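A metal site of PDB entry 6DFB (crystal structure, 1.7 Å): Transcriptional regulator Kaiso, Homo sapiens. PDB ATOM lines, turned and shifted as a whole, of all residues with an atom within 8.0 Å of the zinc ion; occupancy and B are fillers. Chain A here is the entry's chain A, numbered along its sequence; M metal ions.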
ATOM      1  N   GLN A  81      24.819  10.339  -5.032  1.00  0.00           N
ATOM      2  CA  GLN A  81      24.184  11.064  -6.134  1.00  0.00           C
ATOM      3  C   GLN A  81      25.117  11.207  -7.341  1.00  0.00           C
ATOM      4  O   GLN A  81      26.244  11.661  -7.205  1.00  0.00           O
ATOM      5  CB  GLN A  81      23.699  12.447  -5.707  1.00  0.00           C
ATOM      6  CG  GLN A  81      22.922  13.146  -6.825  1.00  0.00           C
ATOM      7  CD  GLN A  81      22.239  14.435  -6.381  1.00  0.00           C
ATOM      8  OE1 GLN A  81      22.684  15.091  -5.433  1.00  0.00           O
ATOM      9  NE2 GLN A  81      21.176  14.819  -7.076  1.00  0.00           N
ATOM     10  N   CYS A  82      24.619  10.810  -8.506  1.00  0.00           N
ATOM     11  CA  CYS A  82      25.351  11.000  -9.762  1.00  0.00           C
ATOM     12  C   CYS A  82      25.376  12.490 -10.111  1.00  0.00           C
ATOM     13  O   CYS A  82      24.307  13.141 -10.176  1.00  0.00           O
ATOM     14  CB  CYS A  82      24.700  10.192 -10.880  1.00  0.00           C
ATOM     15  SG  CYS A  82      25.359  10.487 -12.526  1.00  0.00           S
ATOM     16  N   LEU A  83      26.558  13.045 -10.352  1.00  0.00           N
ATOM     17  CA  LEU A  83      26.669  14.471 -10.644  1.00  0.00           C
ATOM     18  C   LEU A  83      26.407  14.790 -12.119  1.00  0.00           C
ATOM     19  O   LEU A  83      26.168  15.943 -12.472  1.00  0.00           O
ATOM     20  CB  LEU A  83      28.045  15.011 -10.238  1.00  0.00           C
ATOM     21  CG  LEU A  83      28.329  14.945  -8.736  1.00  0.00           C
ATOM     22  CD1 LEU A  83      29.692  15.548  -8.433  1.00  0.00           C
ATOM     23  CD2 LEU A  83      27.237  15.649  -7.940  1.00  0.00           C
ATOM     24  N   ALA A  84      26.447  13.771 -12.966  1.00  0.00           N
ATOM     25  CA  ALA A  84      26.147  13.951 -14.382  1.00  0.00           C
ATOM     26  C   ALA A  84      24.660  14.138 -14.663  1.00  0.00           C
ATOM     27  O   ALA A  84      24.292  14.946 -15.508  1.00  0.00           O
ATOM     28  CB  ALA A  84      26.697  12.771 -15.186  1.00  0.00           C
ATOM     29  N   CYS A  85      23.783  13.412 -13.962  1.00  0.00           N
ATOM     30  CA  CYS A  85      22.355  13.500 -14.252  1.00  0.00           C
ATOM     31  C   CYS A  85      21.478  13.707 -13.012  1.00  0.00           C
ATOM     32  O   CYS A  85      20.269  13.863 -13.139  1.00  0.00           O
ATOM     33  CB  CYS A  85      21.869  12.249 -14.983  1.00  0.00           C
ATOM     34  SG  CYS A  85      21.782  10.754 -13.932  1.00  0.00           S
ATOM     35  N   GLY A  86      22.081  13.666 -11.833  1.00  0.00           N
ATOM     36  CA  GLY A  86      21.346  13.892 -10.591  1.00  0.00           C
ATOM     37  C   GLY A  86      20.608  12.731  -9.951  1.00  0.00           C
ATOM     38  O   GLY A  86      20.093  12.877  -8.846  1.00  0.00           O
ATOM     39  N   LYS A  87      20.559  11.580 -10.621  1.00  0.00           N
ATOM     40  CA  LYS A  87      19.920  10.400 -10.021  1.00  0.00           C
ATOM     41  C   LYS A  87      20.668  10.007  -8.752  1.00  0.00           C
ATOM     42  O   LYS A  87      21.886  10.148  -8.653  1.00  0.00           O
ATOM     43  CB  LYS A  87      19.875   9.208 -10.995  1.00  0.00           C
ATOM     44  CG  LYS A  87      18.920   9.401 -12.183  1.00  0.00           C
ATOM     45  CD  LYS A  87      18.700   8.103 -12.942  1.00  0.00           C
ATOM     46  CE  LYS A  87      17.764   8.320 -14.123  1.00  0.00           C
ATOM     47  NZ  LYS A  87      17.283   7.038 -14.712  1.00  0.00           N
ATOM     48  N   SER A  88      19.920   9.514  -7.773  1.00  0.00           N
ATOM     49  CA  SER A  88      20.500   9.104  -6.487  1.00  0.00           C
ATOM     50  C   SER A  88      20.298   7.615  -6.202  1.00  0.00           C
ATOM     51  O   SER A  88      19.362   6.987  -6.711  1.00  0.00           O
ATOM     52  CB  SER A  88      19.898   9.929  -5.350  1.00  0.00           C
ATOM     53  OG  SER A  88      19.987  11.319  -5.667  1.00  0.00           O
ATOM     54  N   PHE A  89      21.207   7.066  -5.404  1.00  0.00           N
ATOM     55  CA  PHE A  89      21.339   5.615  -5.193  1.00  0.00           C
ATOM     56  C   PHE A  89      21.613   5.299  -3.733  1.00  0.00           C
ATOM     57  O   PHE A  89      22.149   6.127  -3.002  1.00  0.00           O
ATOM     58  CB  PHE A  89      22.460   5.058  -6.094  1.00  0.00           C
ATOM     59  CG  PHE A  89      22.243   5.382  -7.558  1.00  0.00           C
ATOM     60  CD1 PHE A  89      21.426   4.583  -8.341  1.00  0.00           C
ATOM     61  CD2 PHE A  89      22.798   6.519  -8.118  1.00  0.00           C
ATOM     62  CE1 PHE A  89      21.160   4.897  -9.665  1.00  0.00           C
ATOM     63  CE2 PHE A  89      22.536   6.840  -9.437  1.00  0.00           C
ATOM     64  CZ  PHE A  89      21.715   6.025 -10.213  1.00  0.00           C
ATOM     65  N   MET A  95      25.424   3.212  -7.557  1.00  0.00           N
ATOM     66  CA  MET A  95      25.917   4.451  -8.173  1.00  0.00           C
ATOM     67  C   MET A  95      26.940   4.124  -9.266  1.00  0.00           C
ATOM     68  O   MET A  95      26.874   4.657 -10.374  1.00  0.00           O
ATOM     69  CB  MET A  95      26.532   5.371  -7.089  1.00  0.00           C
ATOM     70  CG  MET A  95      27.269   6.650  -7.604  1.00  0.00           C
ATOM     71  SD  MET A  95      28.969   6.291  -8.157  1.00  0.00           S
ATOM     72  CE  MET A  95      29.705   5.677  -6.628  1.00  0.00           C
ATOM     73  N   HIS A  98      25.529   2.470 -12.427  1.00  0.00           N
ATOM     74  CA  HIS A  98      24.861   3.509 -13.186  1.00  0.00           C
ATOM     75  C   HIS A  98      25.841   4.358 -14.002  1.00  0.00           C
ATOM     76  O   HIS A  98      25.660   4.539 -15.205  1.00  0.00           O
ATOM     77  CB  HIS A  98      24.037   4.405 -12.254  1.00  0.00           C
ATOM     78  CG  HIS A  98      23.626   5.691 -12.890  1.00  0.00           C
ATOM     79  ND1 HIS A  98      22.546   5.764 -13.747  1.00  0.00           N
ATOM     80  CD2 HIS A  98      24.156   6.934 -12.826  1.00  0.00           C
ATOM     81  CE1 HIS A  98      22.423   7.011 -14.183  1.00  0.00           C
ATOM     82  NE2 HIS A  98      23.382   7.739 -13.623  1.00  0.00           N
ATOM     83  N   ILE A  99      26.876   4.868 -13.345  1.00  0.00           N
ATOM     84  CA  ILE A  99      27.775   5.802 -14.015  1.00  0.00           C
ATOM     85  C   ILE A  99      28.548   5.076 -15.112  1.00  0.00           C
ATOM     86  O   ILE A  99      28.766   5.619 -16.210  1.00  0.00           O
ATOM     87  CB  ILE A  99      28.706   6.500 -13.004  1.00  0.00           C
ATOM     88  CG1 ILE A  99      27.869   7.417 -12.092  1.00  0.00           C
ATOM     89  CG2 ILE A  99      29.780   7.325 -13.709  1.00  0.00           C
ATOM     90  CD1 ILE A  99      28.696   8.362 -11.234  1.00  0.00           C
ATOM     91  N   LYS A 100      28.913   3.820 -14.859  1.00  0.00           N
ATOM     92  CA  LYS A 100      29.626   3.073 -15.891  1.00  0.00           C
ATOM     93  C   LYS A 100      28.730   2.739 -17.091  1.00  0.00           C
ATOM     94  O   LYS A 100      29.176   2.831 -18.246  1.00  0.00           O
ATOM     95  CB  LYS A 100      30.228   1.788 -15.310  1.00  0.00           C
ATOM     96  CG  LYS A 100      31.377   2.061 -14.345  1.00  0.00           C
ATOM     97  CD  LYS A 100      31.950   0.754 -13.804  1.00  0.00           C
ATOM     98  CE  LYS A 100      33.190   1.030 -12.986  1.00  0.00           C
ATOM     99  NZ  LYS A 100      33.784  -0.244 -12.474  1.00  0.00           N
ATOM    100  N   VAL A 102      25.521   4.069 -17.962  1.00  0.00           N
ATOM    101  CA  VAL A 102      24.824   5.180 -18.601  1.00  0.00           C
ATOM    102  C   VAL A 102      25.777   6.274 -19.094  1.00  0.00           C
ATOM    103  O   VAL A 102      25.561   6.854 -20.159  1.00  0.00           O
ATOM    104  CB  VAL A 102      23.782   5.815 -17.647  1.00  0.00           C
ATOM    105  CG1 VAL A 102      23.128   7.041 -18.295  1.00  0.00           C
ATOM    106  CG2 VAL A 102      22.737   4.775 -17.270  1.00  0.00           C
ATOM    107  N   HIS A 103      26.829   6.548 -18.325  1.00  0.00           N
ATOM    108  CA  HIS A 103      27.711   7.657 -18.678  1.00  0.00           C
ATOM    109  C   HIS A 103      29.067   7.199 -19.215  1.00  0.00           C
ATOM    110  O   HIS A 103      29.857   8.010 -19.685  1.00  0.00           O
ATOM    111  CB  HIS A 103      27.895   8.585 -17.459  1.00  0.00           C
ATOM    112  CG  HIS A 103      26.597   9.130 -16.923  1.00  0.00           C
ATOM    113  ND1 HIS A 103      25.777   9.953 -17.664  1.00  0.00           N
ATOM    114  CD2 HIS A 103      25.972   8.960 -15.732  1.00  0.00           C
ATOM    115  CE1 HIS A 103      24.714  10.267 -16.956  1.00  0.00           C
ATOM    116  NE2 HIS A 103      24.809   9.689 -15.767  1.00  0.00           N
ATOM    117  N   LEU A 113      32.777  12.178  -9.889  1.00  0.00           N
ATOM    118  CA  LEU A 113      31.551  11.936 -10.650  1.00  0.00           C
ATOM    119  C   LEU A 113      30.299  11.747  -9.787  1.00  0.00           C
ATOM    120  O   LEU A 113      29.167  11.715 -10.303  1.00  0.00           O
ATOM    121  CB  LEU A 113      31.746  10.690 -11.519  1.00  0.00           C
ATOM    122  CG  LEU A 113      32.926  10.785 -12.497  1.00  0.00           C
ATOM    123  CD1 LEU A 113      33.004   9.537 -13.356  1.00  0.00           C
ATOM    124  CD2 LEU A 113      32.818  12.031 -13.363  1.00  0.00           C
HETATM  125 ZN    ZN M   1      23.768   9.741 -14.013  1.00  0.00          ZN
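O of Lys 87 lies within hydrogen-bond range of N of Cys 82 (2.8 Å). The side-chain sulfur (SG) of Cys 82 sits close to the backbone NH (N) of Ala 84 (3.5 Å). N of Lys 87 lies close to SG of Cys 85.
Within 4 Å of the zinc ion: Cys 82, Cys 85, His 98 and His 103.
The zinc ion is bound by NE2 of His 103 (2.0 Å), NE2 of His 98 (2.1 Å), SG of Cys 85 (2.2 Å) and SG of Cys 82 (2.3 Å). The zinc ion has four donor atoms within binding distance.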
